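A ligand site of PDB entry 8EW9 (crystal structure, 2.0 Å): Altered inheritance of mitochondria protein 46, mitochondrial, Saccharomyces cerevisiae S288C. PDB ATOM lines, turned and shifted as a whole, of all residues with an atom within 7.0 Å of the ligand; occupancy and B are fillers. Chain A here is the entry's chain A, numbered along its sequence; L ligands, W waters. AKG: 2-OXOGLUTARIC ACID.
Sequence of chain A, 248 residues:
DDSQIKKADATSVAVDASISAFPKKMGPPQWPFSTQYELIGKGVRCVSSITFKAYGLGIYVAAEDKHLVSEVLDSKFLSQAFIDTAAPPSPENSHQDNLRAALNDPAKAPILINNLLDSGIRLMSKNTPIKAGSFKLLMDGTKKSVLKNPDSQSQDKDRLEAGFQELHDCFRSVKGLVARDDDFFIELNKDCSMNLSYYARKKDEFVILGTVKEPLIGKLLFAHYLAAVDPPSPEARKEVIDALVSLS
Phe 135 touches the ligand (CZ to O4, 3.99 Å).
Met 139 touches the ligand.
Thr 142 touches the ligand (OG1 to C3, 3.2 Å).
Phe 171 touches the ligand (CZ to O3, 3.8 Å).
CD2 of His 224 touches O5 of the ligand, 3.96 Å away.
Pro 232 touches the ligand.
Hydrophobic or aromatic side chains that line the ligand: Tyr 55, Phe 135, Met 139, Phe 171, His 224 and Pro 232.
Within 4 Å of the ligand: Arg 45, Tyr 55, Asn 127, Phe 135, Met 139, Thr 142, Phe 171, His 224 and Pro 232.
N of Ala 54 lies within hydrogen-bond range of O of Arg 45.
The side-chain hydroxyl of Tyr 225 lies within hydrogen-bond range of the side-chain amide oxygen of Asn 127 (2.8 Å).
The backbone carbonyl oxygen (O) of Leu 138 lies within hydrogen-bond range of the side-chain hydroxyl (OG1) of Thr 142.
The backbone carbonyl oxygen of Asn 127 is in hydrogen-bond range of the backbone NH of Phe 184 (2.9 Å).
The side-chain hydroxyl of Thr 142 is in hydrogen-bond range of the backbone carbonyl oxygen of Met 139, 3.2 Å away.
O of Tyr 55 is in hydrogen-bond range of N of Arg 45, at 2.8 Å.
ND2 of Asn 127 is in hydrogen-bond range of OG of Ser 125.
OH of Tyr 55 lies within hydrogen-bond range of O2 of the ligand (2.5 Å).
An oxygen (O2) of the ligand is in salt-bridge range of the guanidinium group of Arg 45, 2.8 Å away.
An oxygen (O4) of the ligand sits close to the side-chain amide oxygen (OD1) of Asn 127.
Water W1 lies within hydrogen-bond range of O of Leu 138 (2.7 Å), O1 of the ligand (2.8 Å), OG of Ser 145 (3.1 Å) and O of Gly 141 (3.4 Å).
Water W2 lies within hydrogen-bond range of a ring nitrogen (NE2) of His 224 (2.6 Å), an oxygen (O1) of the ligand (3.1 Å) and the guanidinium group (NH2) of Arg 45 (3.2 Å).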
ATOM      1  N   ARG A  45      11.600  17.774 -24.442  1.00  0.00           N
ATOM      2  CA  ARG A  45      11.485  18.316 -25.792  1.00  0.00           C
ATOM      3  C   ARG A  45      12.821  18.972 -26.106  1.00  0.00           C
ATOM      4  O   ARG A  45      13.182  19.977 -25.487  1.00  0.00           O
ATOM      5  CB  ARG A  45      10.308  19.287 -25.884  1.00  0.00           C
ATOM      6  CG  ARG A  45       9.679  19.442 -27.278  1.00  0.00           C
ATOM      7  CD  ARG A  45      10.607  20.186 -28.235  1.00  0.00           C
ATOM      8  NE  ARG A  45       9.889  20.700 -29.389  1.00  0.00           N
ATOM      9  CZ  ARG A  45      10.454  21.036 -30.544  1.00  0.00           C
ATOM     10  NH1 ARG A  45      11.759  20.888 -30.752  1.00  0.00           N
ATOM     11  NH2 ARG A  45       9.692  21.518 -31.522  1.00  0.00           N
ATOM     12  N   CYS A  46      13.552  18.379 -27.023  1.00  0.00           N
ATOM     13  CA  CYS A  46      14.841  18.846 -27.484  1.00  0.00           C
ATOM     14  C   CYS A  46      14.702  19.514 -28.839  1.00  0.00           C
ATOM     15  O   CYS A  46      13.746  19.305 -29.562  1.00  0.00           O
ATOM     16  CB  CYS A  46      15.810  17.669 -27.601  1.00  0.00           C
ATOM     17  SG  CYS A  46      16.003  16.844 -26.031  1.00  0.00           S
ATOM     18  N   ALA A  54      14.904  21.932 -24.383  1.00  0.00           N
ATOM     19  CA  ALA A  54      14.095  23.150 -24.406  1.00  0.00           C
ATOM     20  C   ALA A  54      13.086  23.190 -23.263  1.00  0.00           C
ATOM     21  O   ALA A  54      13.011  24.193 -22.561  1.00  0.00           O
ATOM     22  CB  ALA A  54      13.385  23.289 -25.747  1.00  0.00           C
ATOM     23  N   TYR A  55      12.330  22.108 -23.063  1.00  0.00           N
ATOM     24  CA  TYR A  55      11.394  22.049 -21.952  1.00  0.00           C
ATOM     25  C   TYR A  55      11.072  20.600 -21.631  1.00  0.00           C
ATOM     26  O   TYR A  55      11.296  19.688 -22.421  1.00  0.00           O
ATOM     27  CB  TYR A  55      10.116  22.843 -22.265  1.00  0.00           C
ATOM     28  CG  TYR A  55       9.198  22.290 -23.341  1.00  0.00           C
ATOM     29  CD1 TYR A  55       9.367  22.625 -24.678  1.00  0.00           C
ATOM     30  CD2 TYR A  55       8.133  21.476 -23.016  1.00  0.00           C
ATOM     31  CE1 TYR A  55       8.506  22.145 -25.662  1.00  0.00           C
ATOM     32  CE2 TYR A  55       7.270  20.983 -23.984  1.00  0.00           C
ATOM     33  CZ  TYR A  55       7.456  21.317 -25.307  1.00  0.00           C
ATOM     34  OH  TYR A  55       6.582  20.815 -26.271  1.00  0.00           O
ATOM     35  N   LEU A  57       8.147  17.932 -20.921  1.00  0.00           N
ATOM     36  CA  LEU A  57       6.753  17.731 -21.320  1.00  0.00           C
ATOM     37  C   LEU A  57       6.114  16.627 -20.488  1.00  0.00           C
ATOM     38  O   LEU A  57       6.679  15.543 -20.349  1.00  0.00           O
ATOM     39  CB  LEU A  57       6.655  17.397 -22.797  1.00  0.00           C
ATOM     40  CG  LEU A  57       5.245  17.116 -23.301  1.00  0.00           C
ATOM     41  CD1 LEU A  57       4.298  18.324 -23.118  1.00  0.00           C
ATOM     42  CD2 LEU A  57       5.265  16.674 -24.747  1.00  0.00           C
ATOM     43  N   SER A 125      -1.556  19.065 -20.902  1.00  0.00           N
ATOM     44  CA  SER A 125      -0.109  19.063 -21.128  1.00  0.00           C
ATOM     45  C   SER A 125       0.511  19.989 -20.099  1.00  0.00           C
ATOM     46  O   SER A 125      -0.007  21.095 -19.864  1.00  0.00           O
ATOM     47  CB  SER A 125       0.269  19.467 -22.550  1.00  0.00           C
ATOM     48  OG  SER A 125       0.136  20.870 -22.762  1.00  0.00           O
ATOM     49  N   ASN A 127       3.972  21.854 -19.565  1.00  0.00           N
ATOM     50  CA  ASN A 127       5.084  22.293 -20.396  1.00  0.00           C
ATOM     51  C   ASN A 127       5.957  23.157 -19.500  1.00  0.00           C
ATOM     52  O   ASN A 127       5.606  24.302 -19.211  1.00  0.00           O
ATOM     53  CB  ASN A 127       4.591  23.042 -21.627  1.00  0.00           C
ATOM     54  CG  ASN A 127       3.472  22.331 -22.326  1.00  0.00           C
ATOM     55  OD1 ASN A 127       3.671  21.576 -23.290  1.00  0.00           O
ATOM     56  ND2 ASN A 127       2.253  22.546 -21.832  1.00  0.00           N
ATOM     57  N   THR A 128       7.084  22.585 -19.065  1.00  0.00           N
ATOM     58  CA  THR A 128       7.977  23.197 -18.087  1.00  0.00           C
ATOM     59  C   THR A 128       9.264  23.628 -18.759  1.00  0.00           C
ATOM     60  O   THR A 128      10.067  22.765 -19.147  1.00  0.00           O
ATOM     61  CB  THR A 128       8.293  22.199 -16.965  1.00  0.00           C
ATOM     62  OG1 THR A 128       7.079  21.806 -16.344  1.00  0.00           O
ATOM     63  CG2 THR A 128       9.262  22.803 -15.919  1.00  0.00           C
ATOM     64  N   PHE A 135      12.198  28.106 -25.471  1.00  0.00           N
ATOM     65  CA  PHE A 135      10.770  27.891 -25.251  1.00  0.00           C
ATOM     66  C   PHE A 135       9.945  28.994 -25.901  1.00  0.00           C
ATOM     67  O   PHE A 135       9.017  28.717 -26.677  1.00  0.00           O
ATOM     68  CB  PHE A 135      10.509  27.808 -23.734  1.00  0.00           C
ATOM     69  CG  PHE A 135       9.130  27.332 -23.383  1.00  0.00           C
ATOM     70  CD1 PHE A 135       8.851  25.979 -23.288  1.00  0.00           C
ATOM     71  CD2 PHE A 135       8.122  28.237 -23.130  1.00  0.00           C
ATOM     72  CE1 PHE A 135       7.595  25.547 -22.977  1.00  0.00           C
ATOM     73  CE2 PHE A 135       6.865  27.798 -22.810  1.00  0.00           C
ATOM     74  CZ  PHE A 135       6.598  26.460 -22.728  1.00  0.00           C
ATOM     75  N   LEU A 138       9.823  28.368 -29.484  1.00  0.00           N
ATOM     76  CA  LEU A 138       8.935  27.271 -29.820  1.00  0.00           C
ATOM     77  C   LEU A 138       7.469  27.695 -29.720  1.00  0.00           C
ATOM     78  O   LEU A 138       6.628  27.186 -30.465  1.00  0.00           O
ATOM     79  CB  LEU A 138       9.202  26.088 -28.907  1.00  0.00           C
ATOM     80  CG  LEU A 138      10.549  25.384 -29.159  1.00  0.00           C
ATOM     81  CD1 LEU A 138      10.753  24.211 -28.195  1.00  0.00           C
ATOM     82  CD2 LEU A 138      10.661  24.913 -30.590  1.00  0.00           C
ATOM     83  N   MET A 139       7.163  28.623 -28.811  1.00  0.00           N
ATOM     84  CA  MET A 139       5.828  29.200 -28.764  1.00  0.00           C
ATOM     85  C   MET A 139       5.512  29.925 -30.069  1.00  0.00           C
ATOM     86  O   MET A 139       4.462  29.683 -30.689  1.00  0.00           O
ATOM     87  CB  MET A 139       5.734  30.136 -27.562  1.00  0.00           C
ATOM     88  CG  MET A 139       5.820  29.444 -26.196  1.00  0.00           C
ATOM     89  SD  MET A 139       5.835  30.617 -24.812  1.00  0.00           S
ATOM     90  CE  MET A 139       4.210  31.363 -24.950  1.00  0.00           C
ATOM     91  N   ASP A 140       6.405  30.815 -30.497  1.00  0.00           N
ATOM     92  CA  ASP A 140       6.198  31.538 -31.737  1.00  0.00           C
ATOM     93  C   ASP A 140       5.962  30.600 -32.907  1.00  0.00           C
ATOM     94  O   ASP A 140       5.209  30.916 -33.838  1.00  0.00           O
ATOM     95  CB  ASP A 140       7.418  32.417 -32.054  1.00  0.00           C
ATOM     96  CG  ASP A 140       7.540  33.617 -31.140  1.00  0.00           C
ATOM     97  OD1 ASP A 140       6.608  33.879 -30.349  1.00  0.00           O
ATOM     98  OD2 ASP A 140       8.583  34.300 -31.211  1.00  0.00           O
ATOM     99  N   GLY A 141       6.626  29.450 -32.900  1.00  0.00           N
ATOM    100  CA  GLY A 141       6.527  28.492 -33.977  1.00  0.00           C
ATOM    101  C   GLY A 141       5.439  27.445 -33.831  1.00  0.00           C
ATOM    102  O   GLY A 141       5.369  26.536 -34.658  1.00  0.00           O
ATOM    103  N   THR A 142       4.588  27.552 -32.808  1.00  0.00           N
ATOM    104  CA  THR A 142       3.594  26.506 -32.558  1.00  0.00           C
ATOM    105  C   THR A 142       2.597  26.395 -33.700  1.00  0.00           C
ATOM    106  O   THR A 142       2.269  25.273 -34.137  1.00  0.00           O
ATOM    107  CB  THR A 142       2.865  26.777 -31.242  1.00  0.00           C
ATOM    108  OG1 THR A 142       3.763  26.595 -30.144  1.00  0.00           O
ATOM    109  CG2 THR A 142       1.690  25.816 -31.076  1.00  0.00           C
ATOM    110  N   SER A 145       4.036  24.732 -36.650  1.00  0.00           N
ATOM    111  CA  SER A 145       4.350  23.331 -36.362  1.00  0.00           C
ATOM    112  C   SER A 145       3.098  22.465 -36.454  1.00  0.00           C
ATOM    113  O   SER A 145       3.089  21.430 -37.141  1.00  0.00           O
ATOM    114  CB  SER A 145       4.973  23.202 -34.972  1.00  0.00           C
ATOM    115  OG  SER A 145       6.162  23.955 -34.865  1.00  0.00           O
ATOM    116  N   VAL A 146       2.023  22.861 -35.768  1.00  0.00           N
ATOM    117  CA  VAL A 146       0.830  22.014 -35.733  1.00  0.00           C
ATOM    118  C   VAL A 146       0.110  22.004 -37.080  1.00  0.00           C
ATOM    119  O   VAL A 146      -0.705  21.107 -37.321  1.00  0.00           O
ATOM    120  CB  VAL A 146      -0.104  22.479 -34.610  1.00  0.00           C
ATOM    121  CG1 VAL A 146       0.633  22.521 -33.274  1.00  0.00           C
ATOM    122  CG2 VAL A 146      -0.691  23.830 -34.924  1.00  0.00           C
ATOM    123  N   PHE A 171      -0.433  33.351 -25.501  1.00  0.00           N
ATOM    124  CA  PHE A 171       1.025  33.234 -25.546  1.00  0.00           C
ATOM    125  C   PHE A 171       1.709  34.565 -25.254  1.00  0.00           C
ATOM    126  O   PHE A 171       2.802  34.590 -24.676  1.00  0.00           O
ATOM    127  CB  PHE A 171       1.479  32.711 -26.909  1.00  0.00           C
ATOM    128  CG  PHE A 171       1.374  31.216 -27.063  1.00  0.00           C
ATOM    129  CD1 PHE A 171       0.675  30.440 -26.167  1.00  0.00           C
ATOM    130  CD2 PHE A 171       2.023  30.589 -28.123  1.00  0.00           C
ATOM    131  CE1 PHE A 171       0.607  29.086 -26.319  1.00  0.00           C
ATOM    132  CE2 PHE A 171       1.953  29.229 -28.267  1.00  0.00           C
ATOM    133  CZ  PHE A 171       1.238  28.471 -27.371  1.00  0.00           C
ATOM    134  N   PHE A 184       3.745  25.884 -17.678  1.00  0.00           N
ATOM    135  CA  PHE A 184       2.705  26.349 -18.602  1.00  0.00           C
ATOM    136  C   PHE A 184       1.736  25.187 -18.819  1.00  0.00           C
ATOM    137  O   PHE A 184       2.119  24.161 -19.409  1.00  0.00           O
ATOM    138  CB  PHE A 184       3.329  26.797 -19.918  1.00  0.00           C
ATOM    139  CG  PHE A 184       2.356  27.359 -20.923  1.00  0.00           C
ATOM    140  CD1 PHE A 184       1.090  27.798 -20.565  1.00  0.00           C
ATOM    141  CD2 PHE A 184       2.725  27.446 -22.255  1.00  0.00           C
ATOM    142  CE1 PHE A 184       0.230  28.308 -21.507  1.00  0.00           C
ATOM    143  CE2 PHE A 184       1.857  27.960 -23.208  1.00  0.00           C
ATOM    144  CZ  PHE A 184       0.612  28.384 -22.833  1.00  0.00           C
ATOM    145  N   ILE A 186      -1.838  23.484 -20.261  1.00  0.00           N
ATOM    146  CA  ILE A 186      -2.822  23.542 -21.329  1.00  0.00           C
ATOM    147  C   ILE A 186      -3.776  22.373 -21.122  1.00  0.00           C
ATOM    148  O   ILE A 186      -3.383  21.212 -21.302  1.00  0.00           O
ATOM    149  CB  ILE A 186      -2.181  23.481 -22.718  1.00  0.00           C
ATOM    150  CG1 ILE A 186      -1.196  24.655 -22.891  1.00  0.00           C
ATOM    151  CG2 ILE A 186      -3.256  23.492 -23.771  1.00  0.00           C
ATOM    152  CD1 ILE A 186      -0.383  24.605 -24.185  1.00  0.00           C
ATOM    153  N   LEU A 221      -3.277  20.769 -31.741  1.00  0.00           N
ATOM    154  CA  LEU A 221      -2.152  20.748 -30.820  1.00  0.00           C
ATOM    155  C   LEU A 221      -1.969  19.374 -30.190  1.00  0.00           C
ATOM    156  O   LEU A 221      -0.850  18.858 -30.112  1.00  0.00           O
ATOM    157  CB  LEU A 221      -2.330  21.821 -29.737  1.00  0.00           C
ATOM    158  CG  LEU A 221      -1.268  21.880 -28.642  1.00  0.00           C
ATOM    159  CD1 LEU A 221       0.104  22.202 -29.250  1.00  0.00           C
ATOM    160  CD2 LEU A 221      -1.669  22.889 -27.564  1.00  0.00           C
ATOM    161  N   HIS A 224      -0.683  16.800 -32.464  1.00  0.00           N
ATOM    162  CA  HIS A 224       0.752  16.972 -32.640  1.00  0.00           C
ATOM    163  C   HIS A 224       1.541  16.347 -31.503  1.00  0.00           C
ATOM    164  O   HIS A 224       2.545  15.652 -31.728  1.00  0.00           O
ATOM    165  CB  HIS A 224       1.081  18.456 -32.763  1.00  0.00           C
ATOM    166  CG  HIS A 224       2.534  18.742 -32.987  1.00  0.00           C
ATOM    167  ND1 HIS A 224       3.244  18.196 -34.037  1.00  0.00           N
ATOM    168  CD2 HIS A 224       3.412  19.507 -32.301  1.00  0.00           C
ATOM    169  CE1 HIS A 224       4.503  18.617 -33.982  1.00  0.00           C
ATOM    170  NE2 HIS A 224       4.628  19.413 -32.943  1.00  0.00           N
ATOM    171  N   TYR A 225       1.130  16.619 -30.247  1.00  0.00           N
ATOM    172  CA  TYR A 225       1.785  16.001 -29.109  1.00  0.00           C
ATOM    173  C   TYR A 225       1.860  14.490 -29.291  1.00  0.00           C
ATOM    174  O   TYR A 225       2.902  13.875 -29.045  1.00  0.00           O
ATOM    175  CB  TYR A 225       1.046  16.306 -27.792  1.00  0.00           C
ATOM    176  CG  TYR A 225       1.260  17.667 -27.136  1.00  0.00           C
ATOM    177  CD1 TYR A 225       2.531  18.133 -26.784  1.00  0.00           C
ATOM    178  CD2 TYR A 225       0.171  18.462 -26.815  1.00  0.00           C
ATOM    179  CE1 TYR A 225       2.690  19.380 -26.163  1.00  0.00           C
ATOM    180  CE2 TYR A 225       0.326  19.699 -26.202  1.00  0.00           C
ATOM    181  CZ  TYR A 225       1.581  20.147 -25.855  1.00  0.00           C
ATOM    182  OH  TYR A 225       1.680  21.374 -25.233  1.00  0.00           O
ATOM    183  N   PRO A 231       6.578  13.857 -33.472  1.00  0.00           N
ATOM    184  CA  PRO A 231       5.988  14.569 -32.337  1.00  0.00           C
ATOM    185  C   PRO A 231       7.038  15.437 -31.661  1.00  0.00           C
ATOM    186  O   PRO A 231       8.238  15.223 -31.858  1.00  0.00           O
ATOM    187  CB  PRO A 231       5.526  13.431 -31.418  1.00  0.00           C
ATOM    188  CG  PRO A 231       6.488  12.329 -31.695  1.00  0.00           C
ATOM    189  CD  PRO A 231       6.798  12.423 -33.172  1.00  0.00           C
ATOM    190  N   PRO A 232       6.626  16.444 -30.883  1.00  0.00           N
ATOM    191  CA  PRO A 232       7.618  17.303 -30.222  1.00  0.00           C
ATOM    192  C   PRO A 232       8.605  16.518 -29.383  1.00  0.00           C
ATOM    193  O   PRO A 232       9.819  16.747 -29.451  1.00  0.00           O
ATOM    194  CB  PRO A 232       6.754  18.239 -29.354  1.00  0.00           C
ATOM    195  CG  PRO A 232       5.410  18.147 -29.917  1.00  0.00           C
ATOM    196  CD  PRO A 232       5.252  16.772 -30.474  1.00  0.00           C
ATOM    197  N   SER A 233       8.090  15.598 -28.580  1.00  0.00           N
ATOM    198  CA  SER A 233       8.901  14.730 -27.741  1.00  0.00           C
ATOM    199  C   SER A 233       8.604  13.297 -28.141  1.00  0.00           C
ATOM    200  O   SER A 233       7.565  12.735 -27.751  1.00  0.00           O
ATOM    201  CB  SER A 233       8.616  14.929 -26.256  1.00  0.00           C
ATOM    202  OG  SER A 233       9.331  13.970 -25.477  1.00  0.00           O
HETATM  203  C1  AKG L   1       6.692  22.305 -29.321  1.00  0.00           C
HETATM  204  O1  AKG L   1       7.176  22.864 -30.396  1.00  0.00           O
HETATM  205  O2  AKG L   1       7.318  21.544 -28.601  1.00  0.00           O
HETATM  206  C2  AKG L   1       5.207  22.632 -29.031  1.00  0.00           C
HETATM  207  O5  AKG L   1       4.327  21.792 -29.195  1.00  0.00           O
HETATM  208  C3  AKG L   1       4.884  24.020 -28.554  1.00  0.00           C
HETATM  209  C4  AKG L   1       3.760  24.049 -27.537  1.00  0.00           C
HETATM  210  C5  AKG L   1       4.153  24.756 -26.289  1.00  0.00           C
HETATM  211  O3  AKG L   1       3.975  26.056 -26.356  1.00  0.00           O
HETATM  212  O4  AKG L   1       4.605  24.181 -25.323  1.00  0.00           O
HETATM  213  O   HOH W   1       7.006  25.083 -32.086  1.00  0.00           O
HETATM  214  O   HOH W   2       6.763  20.877 -32.689  1.00  0.00           O
